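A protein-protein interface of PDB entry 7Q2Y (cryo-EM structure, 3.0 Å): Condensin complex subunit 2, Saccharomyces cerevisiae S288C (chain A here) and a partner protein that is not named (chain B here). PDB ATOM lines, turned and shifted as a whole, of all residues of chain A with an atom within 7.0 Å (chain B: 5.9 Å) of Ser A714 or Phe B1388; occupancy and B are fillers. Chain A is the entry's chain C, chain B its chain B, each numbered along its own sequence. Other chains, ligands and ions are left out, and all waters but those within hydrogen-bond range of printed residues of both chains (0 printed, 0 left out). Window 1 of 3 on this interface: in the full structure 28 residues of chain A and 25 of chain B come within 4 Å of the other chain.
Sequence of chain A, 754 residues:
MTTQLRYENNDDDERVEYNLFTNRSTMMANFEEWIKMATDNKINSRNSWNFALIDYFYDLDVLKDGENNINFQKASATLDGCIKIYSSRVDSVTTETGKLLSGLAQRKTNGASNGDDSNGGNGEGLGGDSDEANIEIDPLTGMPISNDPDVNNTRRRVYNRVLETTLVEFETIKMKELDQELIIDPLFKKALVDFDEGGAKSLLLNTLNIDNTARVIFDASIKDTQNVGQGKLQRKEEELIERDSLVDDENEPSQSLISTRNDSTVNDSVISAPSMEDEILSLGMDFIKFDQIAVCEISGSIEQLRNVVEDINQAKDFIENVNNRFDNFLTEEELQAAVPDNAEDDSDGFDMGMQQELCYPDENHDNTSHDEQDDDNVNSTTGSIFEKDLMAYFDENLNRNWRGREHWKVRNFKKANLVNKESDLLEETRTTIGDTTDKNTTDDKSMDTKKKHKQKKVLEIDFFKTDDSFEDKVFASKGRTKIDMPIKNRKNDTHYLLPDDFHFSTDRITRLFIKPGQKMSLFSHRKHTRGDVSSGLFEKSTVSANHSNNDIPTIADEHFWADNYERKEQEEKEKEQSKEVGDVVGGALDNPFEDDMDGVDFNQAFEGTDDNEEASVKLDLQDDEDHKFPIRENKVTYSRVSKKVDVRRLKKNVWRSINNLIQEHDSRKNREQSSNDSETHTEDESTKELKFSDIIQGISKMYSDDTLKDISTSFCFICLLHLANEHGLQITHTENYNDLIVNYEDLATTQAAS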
ATOM      1  N   LYS A 643     -19.424 -13.198  23.450  1.00  0.00           N
ATOM      2  CA  LYS A 643     -19.691 -12.947  24.860  1.00  0.00           C
ATOM      3  C   LYS A 643     -18.380 -12.717  25.597  1.00  0.00           C
ATOM      4  O   LYS A 643     -17.420 -13.473  25.417  1.00  0.00           O
ATOM      5  CB  LYS A 643     -20.452 -14.118  25.488  1.00  0.00           C
ATOM      6  CG  LYS A 643     -21.687 -14.545  24.709  1.00  0.00           C
ATOM      7  CD  LYS A 643     -22.739 -15.159  25.621  1.00  0.00           C
ATOM      8  CE  LYS A 643     -22.125 -16.163  26.583  1.00  0.00           C
ATOM      9  NZ  LYS A 643     -23.161 -16.835  27.416  1.00  0.00           N
ATOM     10  N   LEU A 650     -14.578 -14.107  37.270  1.00  0.00           N
ATOM     11  CA  LEU A 650     -15.592 -15.067  37.694  1.00  0.00           C
ATOM     12  C   LEU A 650     -15.021 -16.066  38.692  1.00  0.00           C
ATOM     13  O   LEU A 650     -15.661 -16.390  39.698  1.00  0.00           O
ATOM     14  CB  LEU A 650     -16.170 -15.790  36.476  1.00  0.00           C
ATOM     15  CG  LEU A 650     -17.416 -16.643  36.719  1.00  0.00           C
ATOM     16  CD1 LEU A 650     -18.409 -15.915  37.611  1.00  0.00           C
ATOM     17  CD2 LEU A 650     -18.063 -17.034  35.400  1.00  0.00           C
ATOM     18  N   ILE A 711     -23.371 -14.604  32.110  1.00  0.00           N
ATOM     19  CA  ILE A 711     -22.925 -15.736  32.914  1.00  0.00           C
ATOM     20  C   ILE A 711     -23.910 -16.890  32.788  1.00  0.00           C
ATOM     21  O   ILE A 711     -25.132 -16.706  32.875  1.00  0.00           O
ATOM     22  CB  ILE A 711     -22.746 -15.319  34.385  1.00  0.00           C
ATOM     23  CG1 ILE A 711     -21.748 -14.167  34.501  1.00  0.00           C
ATOM     24  CG2 ILE A 711     -22.291 -16.501  35.226  1.00  0.00           C
ATOM     25  CD1 ILE A 711     -20.421 -14.437  33.831  1.00  0.00           C
ATOM     26  N   SER A 712     -23.377 -18.092  32.581  1.00  0.00           N
ATOM     27  CA  SER A 712     -24.163 -19.313  32.512  1.00  0.00           C
ATOM     28  C   SER A 712     -23.631 -20.305  33.537  1.00  0.00           C
ATOM     29  O   SER A 712     -22.558 -20.119  34.116  1.00  0.00           O
ATOM     30  CB  SER A 712     -24.131 -19.924  31.105  1.00  0.00           C
ATOM     31  OG  SER A 712     -24.737 -19.060  30.159  1.00  0.00           O
ATOM     32  N   THR A 713     -24.401 -21.373  33.763  1.00  0.00           N
ATOM     33  CA  THR A 713     -23.994 -22.380  34.739  1.00  0.00           C
ATOM     34  C   THR A 713     -22.752 -23.139  34.285  1.00  0.00           C
ATOM     35  O   THR A 713     -21.993 -23.637  35.124  1.00  0.00           O
ATOM     36  CB  THR A 713     -25.147 -23.349  35.013  1.00  0.00           C
ATOM     37  OG1 THR A 713     -24.793 -24.226  36.091  1.00  0.00           O
ATOM     38  CG2 THR A 713     -25.477 -24.173  33.776  1.00  0.00           C
ATOM     39  N   SER A 714     -22.529 -23.236  32.972  1.00  0.00           N
ATOM     40  CA  SER A 714     -21.340 -23.918  32.471  1.00  0.00           C
ATOM     41  C   SER A 714     -20.069 -23.177  32.869  1.00  0.00           C
ATOM     42  O   SER A 714     -19.066 -23.802  33.234  1.00  0.00           O
ATOM     43  CB  SER A 714     -21.427 -24.067  30.954  1.00  0.00           C
ATOM     44  OG  SER A 714     -21.315 -22.808  30.313  1.00  0.00           O
ATOM     45  N   PHE A 715     -20.091 -21.845  32.801  1.00  0.00           N
ATOM     46  CA  PHE A 715     -18.927 -21.065  33.210  1.00  0.00           C
ATOM     47  C   PHE A 715     -18.647 -21.227  34.698  1.00  0.00           C
ATOM     48  O   PHE A 715     -17.486 -21.331  35.111  1.00  0.00           O
ATOM     49  CB  PHE A 715     -19.132 -19.593  32.859  1.00  0.00           C
ATOM     50  CG  PHE A 715     -18.480 -19.189  31.575  1.00  0.00           C
ATOM     51  CD1 PHE A 715     -17.101 -19.119  31.477  1.00  0.00           C
ATOM     52  CD2 PHE A 715     -19.242 -18.895  30.461  1.00  0.00           C
ATOM     53  CE1 PHE A 715     -16.497 -18.752  30.295  1.00  0.00           C
ATOM     54  CE2 PHE A 715     -18.644 -18.531  29.278  1.00  0.00           C
ATOM     55  CZ  PHE A 715     -17.269 -18.459  29.192  1.00  0.00           C
ATOM     56  N   CYS A 716     -19.698 -21.242  35.519  1.00  0.00           N
ATOM     57  CA  CYS A 716     -19.511 -21.464  36.948  1.00  0.00           C
ATOM     58  C   CYS A 716     -18.953 -22.856  37.218  1.00  0.00           C
ATOM     59  O   CYS A 716     -18.099 -23.031  38.093  1.00  0.00           O
ATOM     60  CB  CYS A 716     -20.830 -21.255  37.687  1.00  0.00           C
ATOM     61  SG  CYS A 716     -21.571 -19.626  37.424  1.00  0.00           S
ATOM     62  N   PHE A 717     -19.422 -23.858  36.470  1.00  0.00           N
ATOM     63  CA  PHE A 717     -18.879 -25.205  36.612  1.00  0.00           C
ATOM     64  C   PHE A 717     -17.401 -25.247  36.240  1.00  0.00           C
ATOM     65  O   PHE A 717     -16.597 -25.886  36.930  1.00  0.00           O
ATOM     66  CB  PHE A 717     -19.680 -26.182  35.750  1.00  0.00           C
ATOM     67  CG  PHE A 717     -19.302 -27.621  35.951  1.00  0.00           C
ATOM     68  CD1 PHE A 717     -19.098 -28.129  37.222  1.00  0.00           C
ATOM     69  CD2 PHE A 717     -19.155 -28.468  34.865  1.00  0.00           C
ATOM     70  CE1 PHE A 717     -18.751 -29.453  37.406  1.00  0.00           C
ATOM     71  CE2 PHE A 717     -18.810 -29.793  35.044  1.00  0.00           C
ATOM     72  CZ  PHE A 717     -18.608 -30.286  36.317  1.00  0.00           C
ATOM     73  N   ILE A 718     -17.024 -24.566  35.156  1.00  0.00           N
ATOM     74  CA  ILE A 718     -15.624 -24.541  34.737  1.00  0.00           C
ATOM     75  C   ILE A 718     -14.764 -23.836  35.781  1.00  0.00           C
ATOM     76  O   ILE A 718     -13.650 -24.278  36.092  1.00  0.00           O
ATOM     77  CB  ILE A 718     -15.494 -23.882  33.351  1.00  0.00           C
ATOM     78  CG1 ILE A 718     -16.128 -24.772  32.280  1.00  0.00           C
ATOM     79  CG2 ILE A 718     -14.034 -23.602  33.022  1.00  0.00           C
ATOM     80  CD1 ILE A 718     -15.769 -24.381  30.862  1.00  0.00           C
ATOM     81  N   CYS A 719     -15.264 -22.729  36.335  1.00  0.00           N
ATOM     82  CA  CYS A 719     -14.518 -22.021  37.371  1.00  0.00           C
ATOM     83  C   CYS A 719     -14.367 -22.872  38.627  1.00  0.00           C
ATOM     84  O   CYS A 719     -13.308 -22.864  39.265  1.00  0.00           O
ATOM     85  CB  CYS A 719     -15.204 -20.695  37.697  1.00  0.00           C
ATOM     86  SG  CYS A 719     -15.112 -19.470  36.371  1.00  0.00           S
ATOM     87  N   LEU A 720     -15.417 -23.609  38.999  1.00  0.00           N
ATOM     88  CA  LEU A 720     -15.321 -24.506  40.145  1.00  0.00           C
ATOM     89  C   LEU A 720     -14.312 -25.617  39.890  1.00  0.00           C
ATOM     90  O   LEU A 720     -13.560 -26.005  40.791  1.00  0.00           O
ATOM     91  CB  LEU A 720     -16.696 -25.087  40.470  1.00  0.00           C
ATOM     92  CG  LEU A 720     -16.833 -25.833  41.798  1.00  0.00           C
ATOM     93  CD1 LEU A 720     -17.012 -24.851  42.945  1.00  0.00           C
ATOM     94  CD2 LEU A 720     -17.992 -26.813  41.744  1.00  0.00           C
ATOM     95  N   LEU A 721     -14.283 -26.147  38.664  1.00  0.00           N
ATOM     96  CA  LEU A 721     -13.288 -27.156  38.317  1.00  0.00           C
ATOM     97  C   LEU A 721     -11.876 -26.591  38.403  1.00  0.00           C
ATOM     98  O   LEU A 721     -10.958 -27.260  38.892  1.00  0.00           O
ATOM     99  CB  LEU A 721     -13.561 -27.702  36.916  1.00  0.00           C
ATOM    100  CG  LEU A 721     -14.811 -28.568  36.756  1.00  0.00           C
ATOM    101  CD1 LEU A 721     -15.285 -28.546  35.313  1.00  0.00           C
ATOM    102  CD2 LEU A 721     -14.543 -29.990  37.217  1.00  0.00           C
ATOM    103  N   ALA B 182     -20.923 -32.810  26.570  1.00  0.00           N
ATOM    104  CA  ALA B 182     -19.674 -32.082  26.396  1.00  0.00           C
ATOM    105  C   ALA B 182     -18.769 -32.334  27.591  1.00  0.00           C
ATOM    106  O   ALA B 182     -19.214 -32.248  28.742  1.00  0.00           O
ATOM    107  CB  ALA B 182     -19.928 -30.582  26.231  1.00  0.00           C
ATOM    108  N   VAL B 184     -15.604 -30.957  29.577  1.00  0.00           N
ATOM    109  CA  VAL B 184     -14.881 -29.707  29.777  1.00  0.00           C
ATOM    110  C   VAL B 184     -13.991 -29.845  31.003  1.00  0.00           C
ATOM    111  O   VAL B 184     -14.250 -30.675  31.881  1.00  0.00           O
ATOM    112  CB  VAL B 184     -15.841 -28.509  29.938  1.00  0.00           C
ATOM    113  CG1 VAL B 184     -16.616 -28.271  28.652  1.00  0.00           C
ATOM    114  CG2 VAL B 184     -16.790 -28.741  31.104  1.00  0.00           C
ATOM    115  N   SER B1382     -14.378 -29.882  24.333  1.00  0.00           N
ATOM    116  CA  SER B1382     -14.309 -28.525  23.817  1.00  0.00           C
ATOM    117  C   SER B1382     -13.793 -27.570  24.880  1.00  0.00           C
ATOM    118  O   SER B1382     -13.911 -27.821  26.082  1.00  0.00           O
ATOM    119  CB  SER B1382     -15.678 -28.046  23.327  1.00  0.00           C
ATOM    120  OG  SER B1382     -15.648 -26.664  23.014  1.00  0.00           O
ATOM    121  N   LEU B1383     -13.217 -26.462  24.410  1.00  0.00           N
ATOM    122  CA  LEU B1383     -12.840 -25.351  25.265  1.00  0.00           C
ATOM    123  C   LEU B1383     -13.454 -24.033  24.815  1.00  0.00           C
ATOM    124  O   LEU B1383     -13.248 -23.014  25.483  1.00  0.00           O
ATOM    125  CB  LEU B1383     -11.312 -25.209  25.325  1.00  0.00           C
ATOM    126  CG  LEU B1383     -10.547 -26.411  25.882  1.00  0.00           C
ATOM    127  CD1 LEU B1383      -9.078 -26.338  25.499  1.00  0.00           C
ATOM    128  CD2 LEU B1383     -10.708 -26.498  27.392  1.00  0.00           C
ATOM    129  N   ARG B1384     -14.194 -24.020  23.710  1.00  0.00           N
ATOM    130  CA  ARG B1384     -14.856 -22.816  23.233  1.00  0.00           C
ATOM    131  C   ARG B1384     -16.240 -22.687  23.855  1.00  0.00           C
ATOM    132  O   ARG B1384     -16.915 -23.681  24.137  1.00  0.00           O
ATOM    133  CB  ARG B1384     -14.960 -22.812  21.708  1.00  0.00           C
ATOM    134  CG  ARG B1384     -13.621 -22.935  21.000  1.00  0.00           C
ATOM    135  CD  ARG B1384     -12.645 -21.867  21.475  1.00  0.00           C
ATOM    136  NE  ARG B1384     -12.875 -20.561  20.866  1.00  0.00           N
ATOM    137  CZ  ARG B1384     -12.852 -20.305  19.563  1.00  0.00           C
ATOM    138  NH1 ARG B1384     -12.543 -21.236  18.676  1.00  0.00           N
ATOM    139  NH2 ARG B1384     -13.127 -19.074  19.141  1.00  0.00           N
ATOM    140  N   ASN B1385     -16.662 -21.435  24.040  1.00  0.00           N
ATOM    141  CA  ASN B1385     -17.802 -21.129  24.899  1.00  0.00           C
ATOM    142  C   ASN B1385     -19.097 -21.729  24.356  1.00  0.00           C
ATOM    143  O   ASN B1385     -19.869 -22.360  25.096  1.00  0.00           O
ATOM    144  CB  ASN B1385     -17.929 -19.611  25.033  1.00  0.00           C
ATOM    145  CG  ASN B1385     -18.940 -19.203  26.068  1.00  0.00           C
ATOM    146  OD1 ASN B1385     -19.576 -20.049  26.687  1.00  0.00           O
ATOM    147  ND2 ASN B1385     -19.116 -17.899  26.247  1.00  0.00           N
ATOM    148  N   ASN B1386     -19.352 -21.539  23.060  1.00  0.00           N
ATOM    149  CA  ASN B1386     -20.643 -21.912  22.490  1.00  0.00           C
ATOM    150  C   ASN B1386     -20.872 -23.415  22.555  1.00  0.00           C
ATOM    151  O   ASN B1386     -22.002 -23.864  22.779  1.00  0.00           O
ATOM    152  CB  ASN B1386     -20.744 -21.413  21.049  1.00  0.00           C
ATOM    153  CG  ASN B1386     -20.379 -19.949  20.910  1.00  0.00           C
ATOM    154  OD1 ASN B1386     -19.205 -19.601  20.777  1.00  0.00           O
ATOM    155  ND2 ASN B1386     -21.382 -19.081  20.943  1.00  0.00           N
ATOM    156  N   MET B1387     -19.816 -24.208  22.368  1.00  0.00           N
ATOM    157  CA  MET B1387     -19.995 -25.655  22.338  1.00  0.00           C
ATOM    158  C   MET B1387     -20.522 -26.177  23.670  1.00  0.00           C
ATOM    159  O   MET B1387     -21.384 -27.063  23.696  1.00  0.00           O
ATOM    160  CB  MET B1387     -18.684 -26.346  21.967  1.00  0.00           C
ATOM    161  CG  MET B1387     -18.821 -27.849  21.793  1.00  0.00           C
ATOM    162  SD  MET B1387     -19.908 -28.294  20.428  1.00  0.00           S
ATOM    163  CE  MET B1387     -18.881 -27.861  19.027  1.00  0.00           C
ATOM    164  N   PHE B1388     -20.023 -25.645  24.788  1.00  0.00           N
ATOM    165  CA  PHE B1388     -20.505 -26.111  26.080  1.00  0.00           C
ATOM    166  C   PHE B1388     -21.637 -25.267  26.662  1.00  0.00           C
ATOM    167  O   PHE B1388     -22.144 -25.613  27.734  1.00  0.00           O
ATOM    168  CB  PHE B1388     -19.351 -26.233  27.096  1.00  0.00           C
ATOM    169  CG  PHE B1388     -18.652 -24.939  27.423  1.00  0.00           C
ATOM    170  CD1 PHE B1388     -19.228 -24.011  28.273  1.00  0.00           C
ATOM    171  CD2 PHE B1388     -17.381 -24.689  26.937  1.00  0.00           C
ATOM    172  CE1 PHE B1388     -18.576 -22.836  28.589  1.00  0.00           C
ATOM    173  CE2 PHE B1388     -16.720 -23.517  27.253  1.00  0.00           C
ATOM    174  CZ  PHE B1388     -17.319 -22.590  28.080  1.00  0.00           C
ATOM    175  N   GLU B1389     -22.053 -24.179  26.006  1.00  0.00           N
ATOM    176  CA  GLU B1389     -23.383 -23.654  26.319  1.00  0.00           C
ATOM    177  C   GLU B1389     -24.485 -24.217  25.431  1.00  0.00           C
ATOM    178  O   GLU B1389     -25.661 -23.938  25.686  1.00  0.00           O
ATOM    179  CB  GLU B1389     -23.447 -22.124  26.255  1.00  0.00           C
ATOM    180  CG  GLU B1389     -22.857 -21.408  27.454  1.00  0.00           C
ATOM    181  CD  GLU B1389     -22.406 -20.004  27.131  1.00  0.00           C
ATOM    182  OE1 GLU B1389     -22.715 -19.520  26.022  1.00  0.00           O
ATOM    183  OE2 GLU B1389     -21.783 -19.364  28.005  1.00  0.00           O
ATOM    184  N   LEU B1390     -24.149 -24.987  24.404  1.00  0.00           N
ATOM    185  CA  LEU B1390     -25.140 -25.707  23.612  1.00  0.00           C
ATOM    186  C   LEU B1390     -25.027 -27.208  23.850  1.00  0.00           C
ATOM    187  O   LEU B1390     -25.080 -28.014  22.919  1.00  0.00           O
ATOM    188  CB  LEU B1390     -25.023 -25.367  22.127  1.00  0.00           C
ATOM    189  CG  LEU B1390     -25.611 -24.029  21.652  1.00  0.00           C
ATOM    190  CD1 LEU B1390     -24.814 -22.814  22.103  1.00  0.00           C
ATOM    191  CD2 LEU B1390     -25.757 -24.032  20.138  1.00  0.00           C
ATOM    192  N   ALA B1391     -24.870 -27.592  25.113  1.00  0.00           N
ATOM    193  CA  ALA B1391     -24.803 -28.984  25.524  1.00  0.00           C
ATOM    194  C   ALA B1391     -25.864 -29.257  26.582  1.00  0.00           C
ATOM    195  O   ALA B1391     -26.175 -28.393  27.405  1.00  0.00           O
ATOM    196  CB  ALA B1391     -23.418 -29.337  26.076  1.00  0.00           C
ATOM    197  N   LEU B1394     -22.905 -32.087  30.920  1.00  0.00           N
ATOM    198  CA  LEU B1394     -21.537 -31.613  31.081  1.00  0.00           C
ATOM    199  C   LEU B1394     -20.766 -32.558  31.989  1.00  0.00           C
ATOM    200  O   LEU B1394     -21.231 -32.898  33.083  1.00  0.00           O
ATOM    201  CB  LEU B1394     -21.508 -30.193  31.652  1.00  0.00           C
ATOM    202  CG  LEU B1394     -22.379 -29.148  30.954  1.00  0.00           C
ATOM    203  CD1 LEU B1394     -22.466 -27.885  31.793  1.00  0.00           C
ATOM    204  CD2 LEU B1394     -21.832 -28.836  29.570  1.00  0.00           C
ATOM    205  N   ASN B1411     -27.171 -29.216  32.282  1.00  0.00           N
ATOM    206  CA  ASN B1411     -26.923 -27.838  31.877  1.00  0.00           C
ATOM    207  C   ASN B1411     -28.121 -26.931  32.138  1.00  0.00           C
ATOM    208  O   ASN B1411     -28.301 -25.924  31.444  1.00  0.00           O
ATOM    209  CB  ASN B1411     -26.530 -27.785  30.402  1.00  0.00           C
ATOM    210  CG  ASN B1411     -25.604 -26.627  30.088  1.00  0.00           C
ATOM    211  OD1 ASN B1411     -25.139 -25.927  30.988  1.00  0.00           O
ATOM    212  ND2 ASN B1411     -25.331 -26.418  28.806  1.00  0.00           N
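The side-chain carboxylate of Glu B1389 lies close to the side-chain amide oxygen of Asn B1385, 2.7 Å away.
ND2 of Asn B1411 sits at hydrogen-bond distance from O of Phe B1388.
The side-chain amide nitrogen of Asn B1411 is in hydrogen-bond range of the backbone carbonyl oxygen of Ala B1391.
SG of Cys A716 lies within hydrogen-bond range of O of Ser A712 (3.5 Å).
The backbone carbonyl oxygen (O) of Phe A715 sits at hydrogen-bond distance from the side-chain sulfur (SG) of Cys A719, 3.3 Å away.
Of the printed residues of chain B, Lys A643 touches Asn B1385 (3.5 Å) and Glu B1389 (2.9 Å).
Of the printed residues of chain B, Ser A712 touches Glu B1389.
Printed residues of chain B within 4 Å of Ser A714: Phe B1388 (3.2 Å) and Glu B1389 (3.5 Å).
Leu A721 touches none of the printed residues of chain B.
Leu B1383 touches none of the printed residues of chain A.
Printed residues of chain A within 4 Å of Asn B1385: Lys A643 and Phe A715.
Phe B1388 touches two residues of chain A.
Printed residues of chain A within 4 Å of Asn B1411: Thr A713.
The nearest residue of chain A that does not touch Phe B1388 is Phe A715 (4.3 Å).
Printed residues of chain B that touch a printed residue of chain A: Asn B1385, Phe B1388, Glu B1389 and Asn B1411.
Hydrophobic or aromatic side chains of chain B that line the printed part of chain A: Phe B1388.
Of the 13 printed residues of chain A, 6 touch a printed residue of chain B.
Hydrophobic or aromatic side chains of chain A that line the printed part of chain B: Phe A715 and Ile A718.
Among the printed residues, Asp or Glu carboxylates within 4 Å of a Lys or Arg side-chain nitrogen of the other chain: Lys A643 with Glu B1389 (2.9 Å).
The side-chain carboxylate of Glu B1389 lies within salt-bridge range of the side-chain amino group of Lys A643 (2.9 Å).
Among the printed residues, merely in contact across the chains: Phe A715 with Asn B1385, Ser A714 with Phe B1388, Thr A713 with Asn B1411, Phe A715 with Glu B1389, Lys A643 with Asn B1385, Ser A714 with Glu B1389, Ile A718 with Phe B1388 and Ser A712 with Glu B1389.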
